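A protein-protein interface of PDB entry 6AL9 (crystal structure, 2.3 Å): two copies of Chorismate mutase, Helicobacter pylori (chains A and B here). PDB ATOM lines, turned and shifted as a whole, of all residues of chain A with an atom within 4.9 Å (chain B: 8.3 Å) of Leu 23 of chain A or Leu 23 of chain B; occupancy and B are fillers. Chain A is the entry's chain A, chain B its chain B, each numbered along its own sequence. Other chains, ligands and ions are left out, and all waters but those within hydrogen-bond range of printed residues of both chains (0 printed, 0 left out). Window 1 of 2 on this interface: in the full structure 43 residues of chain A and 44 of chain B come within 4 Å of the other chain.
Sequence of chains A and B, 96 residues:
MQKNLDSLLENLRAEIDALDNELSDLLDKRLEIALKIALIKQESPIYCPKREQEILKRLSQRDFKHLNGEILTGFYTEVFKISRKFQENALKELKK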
ATOM      1  N   LEU A  19      28.702  16.496  -5.032  1.00  0.00           N
ATOM      2  CA  LEU A  19      28.094  17.451  -5.901  1.00  0.00           C
ATOM      3  C   LEU A  19      27.626  18.635  -5.145  1.00  0.00           C
ATOM      4  O   LEU A  19      27.853  19.722  -5.518  1.00  0.00           O
ATOM      5  CB  LEU A  19      26.893  16.812  -6.547  1.00  0.00           C
ATOM      6  CG  LEU A  19      26.192  17.545  -7.635  1.00  0.00           C
ATOM      7  CD1 LEU A  19      25.633  16.580  -8.642  1.00  0.00           C
ATOM      8  CD2 LEU A  19      25.090  18.278  -6.939  1.00  0.00           C
ATOM      9  N   ASP A  20      26.961  18.390  -4.049  1.00  0.00           N
ATOM     10  CA  ASP A  20      26.427  19.450  -3.224  1.00  0.00           C
ATOM     11  C   ASP A  20      27.512  20.267  -2.570  1.00  0.00           C
ATOM     12  O   ASP A  20      27.330  21.469  -2.395  1.00  0.00           O
ATOM     13  CB  ASP A  20      25.477  18.900  -2.167  1.00  0.00           C
ATOM     14  CG  ASP A  20      24.150  18.491  -2.732  1.00  0.00           C
ATOM     15  OD1 ASP A  20      23.780  18.988  -3.848  1.00  0.00           O
ATOM     16  OD2 ASP A  20      23.489  17.666  -2.048  1.00  0.00           O
ATOM     17  N   ASN A  21      28.651  19.656  -2.231  1.00  0.00           N
ATOM     18  CA  ASN A  21      29.803  20.445  -1.719  1.00  0.00           C
ATOM     19  C   ASN A  21      30.254  21.471  -2.744  1.00  0.00           C
ATOM     20  O   ASN A  21      30.406  22.655  -2.423  1.00  0.00           O
ATOM     21  CB  ASN A  21      31.006  19.575  -1.374  1.00  0.00           C
ATOM     22  CG  ASN A  21      30.754  18.611  -0.212  1.00  0.00           C
ATOM     23  OD1 ASN A  21      29.861  18.804   0.630  1.00  0.00           O
ATOM     24  ND2 ASN A  21      31.533  17.534  -0.193  1.00  0.00           N
ATOM     25  N   GLU A  22      30.455  21.008  -3.977  1.00  0.00           N
ATOM     26  CA  GLU A  22      30.833  21.874  -5.085  1.00  0.00           C
ATOM     27  C   GLU A  22      29.770  22.938  -5.413  1.00  0.00           C
ATOM     28  O   GLU A  22      30.108  24.079  -5.689  1.00  0.00           O
ATOM     29  CB  GLU A  22      31.120  21.026  -6.324  1.00  0.00           C
ATOM     30  CG  GLU A  22      32.324  20.111  -6.187  1.00  0.00           C
ATOM     31  CD  GLU A  22      32.583  19.244  -7.419  1.00  0.00           C
ATOM     32  OE1 GLU A  22      32.272  18.024  -7.389  1.00  0.00           O
ATOM     33  OE2 GLU A  22      33.123  19.773  -8.417  1.00  0.00           O
ATOM     34  N   LEU A  23      28.492  22.556  -5.413  1.00  0.00           N
ATOM     35  CA  LEU A  23      27.409  23.465  -5.782  1.00  0.00           C
ATOM     36  C   LEU A  23      27.336  24.625  -4.761  1.00  0.00           C
ATOM     37  O   LEU A  23      27.200  25.802  -5.105  1.00  0.00           O
ATOM     38  CB  LEU A  23      26.103  22.674  -5.784  1.00  0.00           C
ATOM     39  CG  LEU A  23      24.932  23.077  -6.677  1.00  0.00           C
ATOM     40  CD1 LEU A  23      25.288  23.202  -8.151  1.00  0.00           C
ATOM     41  CD2 LEU A  23      23.828  22.060  -6.503  1.00  0.00           C
ATOM     42  N   SER A  24      27.444  24.265  -3.498  1.00  0.00           N
ATOM     43  CA  SER A  24      27.597  25.245  -2.418  1.00  0.00           C
ATOM     44  C   SER A  24      28.841  26.130  -2.543  1.00  0.00           C
ATOM     45  O   SER A  24      28.753  27.359  -2.381  1.00  0.00           O
ATOM     46  CB  SER A  24      27.666  24.522  -1.077  1.00  0.00           C
ATOM     47  OG  SER A  24      26.533  23.697  -0.929  1.00  0.00           O
ATOM     48  N   ASP A  25      29.993  25.510  -2.786  1.00  0.00           N
ATOM     49  CA  ASP A  25      31.211  26.294  -3.011  1.00  0.00           C
ATOM     50  C   ASP A  25      31.048  27.264  -4.188  1.00  0.00           C
ATOM     51  O   ASP A  25      31.414  28.437  -4.078  1.00  0.00           O
ATOM     52  CB  ASP A  25      32.449  25.410  -3.212  1.00  0.00           C
ATOM     53  CG  ASP A  25      32.966  24.783  -1.889  1.00  0.00           C
ATOM     54  OD1 ASP A  25      32.579  25.244  -0.793  1.00  0.00           O
ATOM     55  OD2 ASP A  25      33.765  23.819  -1.937  1.00  0.00           O
ATOM     56  N   LEU A  26      30.465  26.791  -5.285  1.00  0.00           N
ATOM     57  CA  LEU A  26      30.238  27.667  -6.450  1.00  0.00           C
ATOM     58  C   LEU A  26      29.264  28.812  -6.120  1.00  0.00           C
ATOM     59  O   LEU A  26      29.442  29.935  -6.565  1.00  0.00           O
ATOM     60  CB  LEU A  26      29.718  26.890  -7.663  1.00  0.00           C
ATOM     61  CG  LEU A  26      30.685  26.026  -8.474  1.00  0.00           C
ATOM     62  CD1 LEU A  26      29.938  25.409  -9.639  1.00  0.00           C
ATOM     63  CD2 LEU A  26      31.895  26.785  -9.009  1.00  0.00           C
ATOM     64  N   LEU A  27      28.249  28.534  -5.323  1.00  0.00           N
ATOM     65  CA  LEU A  27      27.274  29.584  -4.966  1.00  0.00           C
ATOM     66  C   LEU A  27      27.896  30.648  -4.055  1.00  0.00           C
ATOM     67  O   LEU A  27      27.623  31.834  -4.181  1.00  0.00           O
ATOM     68  CB  LEU A  27      26.029  28.970  -4.326  1.00  0.00           C
ATOM     69  CG  LEU A  27      24.981  29.990  -3.869  1.00  0.00           C
ATOM     70  CD1 LEU A  27      24.324  30.649  -5.076  1.00  0.00           C
ATOM     71  CD2 LEU A  27      23.963  29.278  -2.986  1.00  0.00           C
ATOM     72  N   ARG A  30      29.886  32.891  -6.157  1.00  0.00           N
ATOM     73  CA  ARG A  30      29.033  33.713  -7.001  1.00  0.00           C
ATOM     74  C   ARG A  30      28.469  34.880  -6.205  1.00  0.00           C
ATOM     75  O   ARG A  30      28.255  35.977  -6.766  1.00  0.00           O
ATOM     76  CB  ARG A  30      27.911  32.876  -7.615  1.00  0.00           C
ATOM     77  CG  ARG A  30      27.143  33.560  -8.728  1.00  0.00           C
ATOM     78  CD  ARG A  30      25.837  32.826  -9.006  1.00  0.00           C
ATOM     79  NE  ARG A  30      25.267  33.170 -10.299  1.00  0.00           N
ATOM     80  CZ  ARG A  30      24.525  34.248 -10.527  1.00  0.00           C
ATOM     81  NH1 ARG A  30      24.245  35.118  -9.550  1.00  0.00           N
ATOM     82  NH2 ARG A  30      24.060  34.459 -11.751  1.00  0.00           N
ATOM     83  N   PHE A  75      15.333  27.429 -10.872  1.00  0.00           N
ATOM     84  CA  PHE A  75      16.612  27.520 -10.222  1.00  0.00           C
ATOM     85  C   PHE A  75      17.081  28.973 -10.094  1.00  0.00           C
ATOM     86  O   PHE A  75      17.343  29.452  -8.985  1.00  0.00           O
ATOM     87  CB  PHE A  75      17.625  26.708 -10.983  1.00  0.00           C
ATOM     88  CG  PHE A  75      18.953  26.587 -10.292  1.00  0.00           C
ATOM     89  CD1 PHE A  75      19.061  25.956  -9.070  1.00  0.00           C
ATOM     90  CD2 PHE A  75      20.098  27.054 -10.896  1.00  0.00           C
ATOM     91  CE1 PHE A  75      20.295  25.825  -8.443  1.00  0.00           C
ATOM     92  CE2 PHE A  75      21.330  26.945 -10.283  1.00  0.00           C
ATOM     93  CZ  PHE A  75      21.429  26.324  -9.057  1.00  0.00           C
ATOM     94  N   TYR A  76      17.175  29.675 -11.222  1.00  0.00           N
ATOM     95  CA  TYR A  76      17.797  30.982 -11.234  1.00  0.00           C
ATOM     96  C   TYR A  76      16.938  32.065 -10.639  1.00  0.00           C
ATOM     97  O   TYR A  76      17.479  33.037 -10.135  1.00  0.00           O
ATOM     98  CB  TYR A  76      18.334  31.362 -12.629  1.00  0.00           C
ATOM     99  CG  TYR A  76      19.752  30.867 -12.780  1.00  0.00           C
ATOM    100  CD1 TYR A  76      20.805  31.557 -12.201  1.00  0.00           C
ATOM    101  CD2 TYR A  76      20.029  29.657 -13.400  1.00  0.00           C
ATOM    102  CE1 TYR A  76      22.097  31.080 -12.274  1.00  0.00           C
ATOM    103  CE2 TYR A  76      21.319  29.189 -13.486  1.00  0.00           C
ATOM    104  CZ  TYR A  76      22.346  29.909 -12.911  1.00  0.00           C
ATOM    105  OH  TYR A  76      23.641  29.451 -12.971  1.00  0.00           O
ATOM    106  N   ILE B  16      30.895  35.561 -13.175  1.00  0.00           N
ATOM    107  CA  ILE B  16      29.510  35.063 -12.989  1.00  0.00           C
ATOM    108  C   ILE B  16      29.102  34.038 -14.061  1.00  0.00           C
ATOM    109  O   ILE B  16      28.627  32.970 -13.743  1.00  0.00           O
ATOM    110  CB  ILE B  16      28.504  36.227 -13.055  1.00  0.00           C
ATOM    111  CG1 ILE B  16      28.684  37.166 -11.857  1.00  0.00           C
ATOM    112  CG2 ILE B  16      27.074  35.736 -13.185  1.00  0.00           C
ATOM    113  CD1 ILE B  16      28.241  36.642 -10.515  1.00  0.00           C
ATOM    114  N   ASP B  17      29.313  34.370 -15.325  1.00  0.00           N
ATOM    115  CA  ASP B  17      28.935  33.502 -16.449  1.00  0.00           C
ATOM    116  C   ASP B  17      29.622  32.139 -16.366  1.00  0.00           C
ATOM    117  O   ASP B  17      29.024  31.094 -16.641  1.00  0.00           O
ATOM    118  CB  ASP B  17      29.331  34.164 -17.798  1.00  0.00           C
ATOM    119  CG  ASP B  17      28.448  35.342 -18.195  1.00  0.00           C
ATOM    120  OD1 ASP B  17      27.411  35.650 -17.551  1.00  0.00           O
ATOM    121  OD2 ASP B  17      28.806  35.978 -19.202  1.00  0.00           O
ATOM    122  N   ALA B  18      30.908  32.144 -16.027  1.00  0.00           N
ATOM    123  CA  ALA B  18      31.665  30.888 -15.873  1.00  0.00           C
ATOM    124  C   ALA B  18      31.110  30.092 -14.707  1.00  0.00           C
ATOM    125  O   ALA B  18      31.019  28.867 -14.773  1.00  0.00           O
ATOM    126  CB  ALA B  18      33.150  31.170 -15.643  1.00  0.00           C
ATOM    127  N   LEU B  19      30.761  30.801 -13.642  1.00  0.00           N
ATOM    128  CA  LEU B  19      30.096  30.197 -12.486  1.00  0.00           C
ATOM    129  C   LEU B  19      28.792  29.556 -12.885  1.00  0.00           C
ATOM    130  O   LEU B  19      28.513  28.438 -12.511  1.00  0.00           O
ATOM    131  CB  LEU B  19      29.834  31.243 -11.399  1.00  0.00           C
ATOM    132  CG  LEU B  19      30.961  31.259 -10.360  1.00  0.00           C
ATOM    133  CD1 LEU B  19      31.045  32.569  -9.611  1.00  0.00           C
ATOM    134  CD2 LEU B  19      30.759  30.126  -9.376  1.00  0.00           C
ATOM    135  N   ASP B  20      28.015  30.271 -13.676  1.00  0.00           N
ATOM    136  CA  ASP B  20      26.727  29.784 -14.086  1.00  0.00           C
ATOM    137  C   ASP B  20      26.799  28.581 -15.015  1.00  0.00           C
ATOM    138  O   ASP B  20      25.966  27.722 -14.918  1.00  0.00           O
ATOM    139  CB  ASP B  20      25.891  30.898 -14.694  1.00  0.00           C
ATOM    140  CG  ASP B  20      25.383  31.875 -13.648  1.00  0.00           C
ATOM    141  OD1 ASP B  20      25.278  31.475 -12.469  1.00  0.00           O
ATOM    142  OD2 ASP B  20      25.066  33.038 -13.997  1.00  0.00           O
ATOM    143  N   ASN B  21      27.792  28.503 -15.893  1.00  0.00           N
ATOM    144  CA  ASN B  21      28.057  27.271 -16.677  1.00  0.00           C
ATOM    145  C   ASN B  21      28.334  26.077 -15.785  1.00  0.00           C
ATOM    146  O   ASN B  21      27.752  25.013 -15.964  1.00  0.00           O
ATOM    147  CB  ASN B  21      29.269  27.444 -17.596  1.00  0.00           C
ATOM    148  CG  ASN B  21      29.015  28.419 -18.762  1.00  0.00           C
ATOM    149  OD1 ASN B  21      27.914  28.926 -18.988  1.00  0.00           O
ATOM    150  ND2 ASN B  21      30.062  28.686 -19.490  1.00  0.00           N
ATOM    151  N   GLU B  22      29.214  26.249 -14.812  1.00  0.00           N
ATOM    152  CA  GLU B  22      29.524  25.181 -13.873  1.00  0.00           C
ATOM    153  C   GLU B  22      28.328  24.793 -12.990  1.00  0.00           C
ATOM    154  O   GLU B  22      28.055  23.626 -12.768  1.00  0.00           O
ATOM    155  CB  GLU B  22      30.704  25.584 -12.991  1.00  0.00           C
ATOM    156  CG  GLU B  22      32.018  25.660 -13.756  1.00  0.00           C
ATOM    157  CD  GLU B  22      33.233  25.779 -12.842  1.00  0.00           C
ATOM    158  OE1 GLU B  22      33.904  26.841 -12.895  1.00  0.00           O
ATOM    159  OE2 GLU B  22      33.515  24.816 -12.077  1.00  0.00           O
ATOM    160  N   LEU B  23      27.620  25.789 -12.498  1.00  0.00           N
ATOM    161  CA  LEU B  23      26.490  25.572 -11.610  1.00  0.00           C
ATOM    162  C   LEU B  23      25.391  24.844 -12.335  1.00  0.00           C
ATOM    163  O   LEU B  23      24.766  23.937 -11.791  1.00  0.00           O
ATOM    164  CB  LEU B  23      25.964  26.936 -11.156  1.00  0.00           C
ATOM    165  CG  LEU B  23      25.494  27.168  -9.717  1.00  0.00           C
ATOM    166  CD1 LEU B  23      26.501  26.747  -8.665  1.00  0.00           C
ATOM    167  CD2 LEU B  23      25.210  28.663  -9.565  1.00  0.00           C
ATOM    168  N   SER B  24      25.145  25.260 -13.571  1.00  0.00           N
ATOM    169  CA  SER B  24      24.217  24.578 -14.477  1.00  0.00           C
ATOM    170  C   SER B  24      24.641  23.147 -14.741  1.00  0.00           C
ATOM    171  O   SER B  24      23.816  22.248 -14.698  1.00  0.00           O
ATOM    172  CB  SER B  24      24.212  25.268 -15.855  1.00  0.00           C
ATOM    173  OG  SER B  24      23.619  26.523 -15.775  1.00  0.00           O
ATOM    174  N   ASP B  25      25.903  22.961 -15.122  1.00  0.00           N
ATOM    175  CA  ASP B  25      26.381  21.617 -15.431  1.00  0.00           C
ATOM    176  C   ASP B  25      26.291  20.745 -14.186  1.00  0.00           C
ATOM    177  O   ASP B  25      25.891  19.591 -14.283  1.00  0.00           O
ATOM    178  CB  ASP B  25      27.805  21.625 -15.975  1.00  0.00           C
ATOM    179  CG  ASP B  25      27.898  22.171 -17.413  1.00  0.00           C
ATOM    180  OD1 ASP B  25      26.945  22.020 -18.216  1.00  0.00           O
ATOM    181  OD2 ASP B  25      28.949  22.774 -17.745  1.00  0.00           O
ATOM    182  N   LEU B  26      26.649  21.277 -13.013  1.00  0.00           N
ATOM    183  CA  LEU B  26      26.559  20.478 -11.786  1.00  0.00           C
ATOM    184  C   LEU B  26      25.124  20.132 -11.453  1.00  0.00           C
ATOM    185  O   LEU B  26      24.859  19.036 -10.996  1.00  0.00           O
ATOM    186  CB  LEU B  26      27.184  21.187 -10.583  1.00  0.00           C
ATOM    187  CG  LEU B  26      28.697  21.188 -10.447  1.00  0.00           C
ATOM    188  CD1 LEU B  26      29.057  21.891  -9.147  1.00  0.00           C
ATOM    189  CD2 LEU B  26      29.234  19.775 -10.433  1.00  0.00           C
ATOM    190  N   LEU B  27      24.195  21.059 -11.692  1.00  0.00           N
ATOM    191  CA  LEU B  27      22.769  20.776 -11.441  1.00  0.00           C
ATOM    192  C   LEU B  27      22.238  19.700 -12.383  1.00  0.00           C
ATOM    193  O   LEU B  27      21.451  18.857 -11.990  1.00  0.00           O
ATOM    194  CB  LEU B  27      21.901  22.044 -11.546  1.00  0.00           C
ATOM    195  CG  LEU B  27      20.422  21.822 -11.274  1.00  0.00           C
ATOM    196  CD1 LEU B  27      20.187  21.506  -9.823  1.00  0.00           C
ATOM    197  CD2 LEU B  27      19.627  23.034 -11.670  1.00  0.00           C
ATOM    198  N   ASP B  28      22.677  19.750 -13.629  1.00  0.00           N
ATOM    199  CA  ASP B  28      22.357  18.730 -14.598  1.00  0.00           C
ATOM    200  C   ASP B  28      22.829  17.339 -14.156  1.00  0.00           C
ATOM    201  O   ASP B  28      22.096  16.362 -14.271  1.00  0.00           O
ATOM    202  CB  ASP B  28      22.963  19.115 -15.952  1.00  0.00           C
ATOM    203  CG  ASP B  28      22.244  18.457 -17.124  1.00  0.00           C
ATOM    204  OD1 ASP B  28      20.996  18.441 -17.124  1.00  0.00           O
ATOM    205  OD2 ASP B  28      22.929  17.977 -18.052  1.00  0.00           O
ATOM    206  N   LYS B  29      24.056  17.256 -13.647  1.00  0.00           N
ATOM    207  CA  LYS B  29      24.617  15.982 -13.151  1.00  0.00           C
ATOM    208  C   LYS B  29      23.856  15.508 -11.938  1.00  0.00           C
ATOM    209  O   LYS B  29      23.713  14.307 -11.721  1.00  0.00           O
ATOM    210  CB  LYS B  29      26.091  16.142 -12.756  1.00  0.00           C
ATOM    211  CG  LYS B  29      27.092  16.050 -13.898  1.00  0.00           C
ATOM    212  CD  LYS B  29      28.115  17.198 -13.894  1.00  0.00           C
ATOM    213  CE  LYS B  29      29.439  16.813 -14.547  1.00  0.00           C
ATOM    214  NZ  LYS B  29      30.254  15.946 -13.641  1.00  0.00           N
ATOM    215  N   ARG B  30      23.369  16.456 -11.137  1.00  0.00           N
ATOM    216  CA  ARG B  30      22.640  16.112  -9.913  1.00  0.00           C
ATOM    217  C   ARG B  30      21.276  15.545 -10.230  1.00  0.00           C
ATOM    218  O   ARG B  30      20.748  14.700  -9.502  1.00  0.00           O
ATOM    219  CB  ARG B  30      22.530  17.310  -8.961  1.00  0.00           C
ATOM    220  CG  ARG B  30      22.101  16.946  -7.551  1.00  0.00           C
ATOM    221  CD  ARG B  30      21.683  18.204  -6.789  1.00  0.00           C
ATOM    222  NE  ARG B  30      21.749  18.059  -5.341  1.00  0.00           N
ATOM    223  CZ  ARG B  30      20.853  17.396  -4.614  1.00  0.00           C
ATOM    224  NH1 ARG B  30      19.783  16.847  -5.190  1.00  0.00           N
ATOM    225  NH2 ARG B  30      20.995  17.308  -3.298  1.00  0.00           N
ATOM    226  N   LEU B  59      25.967  20.487   5.150  1.00  0.00           N
ATOM    227  CA  LEU B  59      26.446  21.696   4.430  1.00  0.00           C
ATOM    228  C   LEU B  59      26.563  22.952   5.311  1.00  0.00           C
ATOM    229  O   LEU B  59      27.465  23.768   5.114  1.00  0.00           O
ATOM    230  CB  LEU B  59      25.535  22.026   3.236  1.00  0.00           C
ATOM    231  CG  LEU B  59      25.519  20.991   2.135  1.00  0.00           C
ATOM    232  CD1 LEU B  59      24.275  21.188   1.277  1.00  0.00           C
ATOM    233  CD2 LEU B  59      26.800  21.060   1.315  1.00  0.00           C
ATOM    234  N   ARG B  62      29.938  23.555   7.061  1.00  0.00           N
ATOM    235  CA  ARG B  62      31.120  23.820   6.238  1.00  0.00           C
ATOM    236  C   ARG B  62      31.505  25.303   6.234  1.00  0.00           C
ATOM    237  O   ARG B  62      30.720  26.164   6.645  1.00  0.00           O
ATOM    238  CB  ARG B  62      30.878  23.355   4.811  1.00  0.00           C
ATOM    239  CG  ARG B  62      30.450  21.902   4.690  1.00  0.00           C
ATOM    240  CD  ARG B  62      30.239  21.487   3.235  1.00  0.00           C
ATOM    241  NE  ARG B  62      31.495  21.192   2.540  1.00  0.00           N
ATOM    242  CZ  ARG B  62      31.901  21.757   1.400  1.00  0.00           C
ATOM    243  NH1 ARG B  62      31.165  22.666   0.771  1.00  0.00           N
ATOM    244  NH2 ARG B  62      33.060  21.399   0.869  1.00  0.00           N
ATOM    245  N   PHE B  64      32.280  28.828   4.698  1.00  0.00           N
ATOM    246  CA  PHE B  64      31.919  29.663   3.550  1.00  0.00           C
ATOM    247  C   PHE B  64      32.158  31.116   3.874  1.00  0.00           C
ATOM    248  O   PHE B  64      31.971  31.512   5.003  1.00  0.00           O
ATOM    249  CB  PHE B  64      30.422  29.516   3.227  1.00  0.00           C
ATOM    250  CG  PHE B  64      30.026  28.140   2.774  1.00  0.00           C
ATOM    251  CD1 PHE B  64      30.524  27.614   1.597  1.00  0.00           C
ATOM    252  CD2 PHE B  64      29.139  27.381   3.526  1.00  0.00           C
ATOM    253  CE1 PHE B  64      30.162  26.353   1.189  1.00  0.00           C
ATOM    254  CE2 PHE B  64      28.766  26.130   3.113  1.00  0.00           C
ATOM    255  CZ  PHE B  64      29.278  25.612   1.949  1.00  0.00           C
ATOM    256  N   LEU B  67      27.845  32.131   2.556  1.00  0.00           N
ATOM    257  CA  LEU B  67      26.674  31.286   2.766  1.00  0.00           C
ATOM    258  C   LEU B  67      26.445  31.189   4.262  1.00  0.00           C
ATOM    259  O   LEU B  67      27.393  31.083   5.023  1.00  0.00           O
ATOM    260  CB  LEU B  67      26.871  29.881   2.185  1.00  0.00           C
ATOM    261  CG  LEU B  67      27.010  29.727   0.667  1.00  0.00           C
ATOM    262  CD1 LEU B  67      26.923  28.258   0.267  1.00  0.00           C
ATOM    263  CD2 LEU B  67      25.996  30.570  -0.085  1.00  0.00           C
ATOM    264  N   LEU B  72      21.392  28.782   2.408  1.00  0.00           N
ATOM    265  CA  LEU B  72      21.395  27.365   2.014  1.00  0.00           C
ATOM    266  C   LEU B  72      19.982  26.812   1.977  1.00  0.00           C
ATOM    267  O   LEU B  72      19.632  26.106   1.029  1.00  0.00           O
ATOM    268  CB  LEU B  72      22.274  26.512   2.933  1.00  0.00           C
ATOM    269  CG  LEU B  72      23.788  26.569   2.673  1.00  0.00           C
ATOM    270  CD1 LEU B  72      24.610  26.146   3.880  1.00  0.00           C
ATOM    271  CD2 LEU B  72      24.176  25.740   1.465  1.00  0.00           C
ATOM    272  N   PHE B  75      18.316  28.277  -1.142  1.00  0.00           N
ATOM    273  CA  PHE B  75      18.906  27.590  -2.263  1.00  0.00           C
ATOM    274  C   PHE B  75      18.390  26.136  -2.424  1.00  0.00           C
ATOM    275  O   PHE B  75      17.909  25.734  -3.495  1.00  0.00           O
ATOM    276  CB  PHE B  75      20.419  27.594  -2.130  1.00  0.00           C
ATOM    277  CG  PHE B  75      21.136  27.108  -3.363  1.00  0.00           C
ATOM    278  CD1 PHE B  75      21.044  27.809  -4.547  1.00  0.00           C
ATOM    279  CD2 PHE B  75      21.901  25.955  -3.327  1.00  0.00           C
ATOM    280  CE1 PHE B  75      21.723  27.385  -5.690  1.00  0.00           C
ATOM    281  CE2 PHE B  75      22.564  25.514  -4.456  1.00  0.00           C
ATOM    282  CZ  PHE B  75      22.483  26.231  -5.645  1.00  0.00           C
ATOM    283  N   TYR B  76      18.507  25.344  -1.361  1.00  0.00           N
ATOM    284  CA  TYR B  76      18.219  23.924  -1.473  1.00  0.00           C
ATOM    285  C   TYR B  76      16.759  23.611  -1.462  1.00  0.00           C
ATOM    286  O   TYR B  76      16.375  22.591  -1.964  1.00  0.00           O
ATOM    287  CB  TYR B  76      18.994  23.089  -0.451  1.00  0.00           C
ATOM    288  CG  TYR B  76      20.339  22.675  -1.014  1.00  0.00           C
ATOM    289  CD1 TYR B  76      20.443  21.603  -1.891  1.00  0.00           C
ATOM    290  CD2 TYR B  76      21.489  23.411  -0.743  1.00  0.00           C
ATOM    291  CE1 TYR B  76      21.650  21.240  -2.436  1.00  0.00           C
ATOM    292  CE2 TYR B  76      22.698  23.050  -1.283  1.00  0.00           C
ATOM    293  CZ  TYR B  76      22.762  21.966  -2.125  1.00  0.00           C
ATOM    294  OH  TYR B  76      23.960  21.606  -2.676  1.00  0.00           O
ATOM    295  N   VAL B  79      16.354  23.610  -5.096  1.00  0.00           N
ATOM    296  CA  VAL B  79      17.043  22.420  -5.572  1.00  0.00           C
ATOM    297  C   VAL B  79      16.305  21.106  -5.287  1.00  0.00           C
ATOM    298  O   VAL B  79      16.207  20.237  -6.169  1.00  0.00           O
ATOM    299  CB  VAL B  79      18.473  22.336  -5.005  1.00  0.00           C
ATOM    300  CG1 VAL B  79      19.129  21.017  -5.385  1.00  0.00           C
ATOM    301  CG2 VAL B  79      19.305  23.475  -5.558  1.00  0.00           C
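Among the printed residues, merely in contact across the chains: Leu 26 of chain A with Leu 19 of chain B (3.1 Å), Leu 19 of chain A with Arg 30 of chain B (3.2 Å), Asp 25 of chain A with Phe 64 of chain B (3.3 Å), Ser 24 of chain A with Leu 67 of chain B (3.3 Å), Leu 26 of chain A with Leu 23 of chain B (3.4 Å), Leu 26 of chain A with Glu 22 of chain B (3.4 Å), Phe 75 of chain A with Phe 75 of chain B (3.5 Å), Ser 24 of chain A with Leu 59 of chain B (3.5 Å), Arg 30 of chain A with Leu 19 of chain B (3.5 Å), Leu 19 of chain A with Leu 26 of chain B (3.5 Å), Arg 30 of chain A with Ile 16 of chain B (3.6 Å), Leu 27 of chain A with Phe 75 of chain B (3.6 Å), Ser 24 of chain A with Phe 64 of chain B (3.6 Å), Glu 22 of chain A with Leu 26 of chain B (3.6 Å), Leu 26 of chain A with Leu 26 of chain B (3.7 Å), Leu 23 of chain A with Leu 26 of chain B (3.7 Å), Ser 24 of chain A with Tyr 76 of chain B (3.7 Å), Leu 23 of chain A with Leu 23 of chain B (3.7 Å), Asp 20 of chain A with Leu 59 of chain B (3.8 Å), Leu 27 of chain A with Leu 67 of chain B (3.8 Å), Tyr 76 of chain A with Leu 23 of chain B (3.8 Å), Phe 75 of chain A with Val 79 of chain B (3.9 Å), Leu 23 of chain A with Tyr 76 of chain B (3.9 Å), Asn 21 of chain A with Leu 59 of chain B (3.9 Å), Phe 75 of chain A with Leu 27 of chain B (3.9 Å), Leu 19 of chain A with Lys 29 of chain B (3.9 Å) and Ser 24 of chain A with Leu 72 of chain B (3.9 Å).
Of chain A, only Leu 23, Leu 26 and Tyr 76 come within 4 Å of Leu 23 of chain B.
Of chain B, only Leu 59, Phe 64, Leu 67, Leu 72 and Tyr 76 come within 4 Å of Ser 24 of chain A.
Of the printed residues of chain B, Arg 30 of chain A touches Ile 16 (3.6 Å), Leu 19 (3.5 Å) and Asp 20 (2.8 Å).
Asp 28 of chain B touches none of the printed residues of chain A.
Asp 25 of chain B touches none of the printed residues of chain A.
The nearest residue of chain B that does not touch Leu 23 of chain A is Phe 75 of chain B (4.1 Å).
The nearest printed residue of chain B that does not touch Leu 19 of chain A is Tyr 76 of chain B (5.2 Å).
Of the 23 printed residues of chain B, 17 touch a printed residue of chain A.
Printed residues of chain A that touch a printed residue of chain B: Leu 19, Asp 20, Asn 21, Glu 22, Leu 23, Ser 24, Asp 25, Leu 26, Leu 27, Arg 30, Phe 75 and Tyr 76.
Glu 22 of chain A touches Leu 26 of chain B, and with the chains exchanged Leu 26 of chain A touches Glu 22 of chain B.
Leu 27 of chain A touches Phe 75 of chain B, and with the chains exchanged Phe 75 of chain A touches Leu 27 of chain B.
NE of Arg 30 of chain B lies within salt-bridge range of OD1 of Asp 20 of chain A.
The side-chain hydroxyl (OH) of Tyr 76 of chain B is in hydrogen-bond range of the side-chain carboxylate (OD1) of Asp 20 of chain A.
O of Asn 21 of chain A is in hydrogen-bond range of NH1 of Arg 62 of chain B (3.3 Å).
The side-chain carboxylate (OD1) of Asp 25 of chain A lies within salt-bridge range of the guanidinium group (NH1) of Arg 62 of chain B (3.3 Å).
NE of Arg 30 of chain A lies within salt-bridge range of OD1 of Asp 20 of chain B, 2.8 Å away.
The side-chain hydroxyl (OH) of Tyr 76 of chain A is in hydrogen-bond range of the side-chain carboxylate (OD1) of Asp 20 of chain B (2.7 Å).
O of Asp 20 of chain A sits at hydrogen-bond distance from OG of Ser 24 of chain A.
O of Asp 20 of chain B sits at hydrogen-bond distance from OG of Ser 24 of chain B (2.8 Å).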
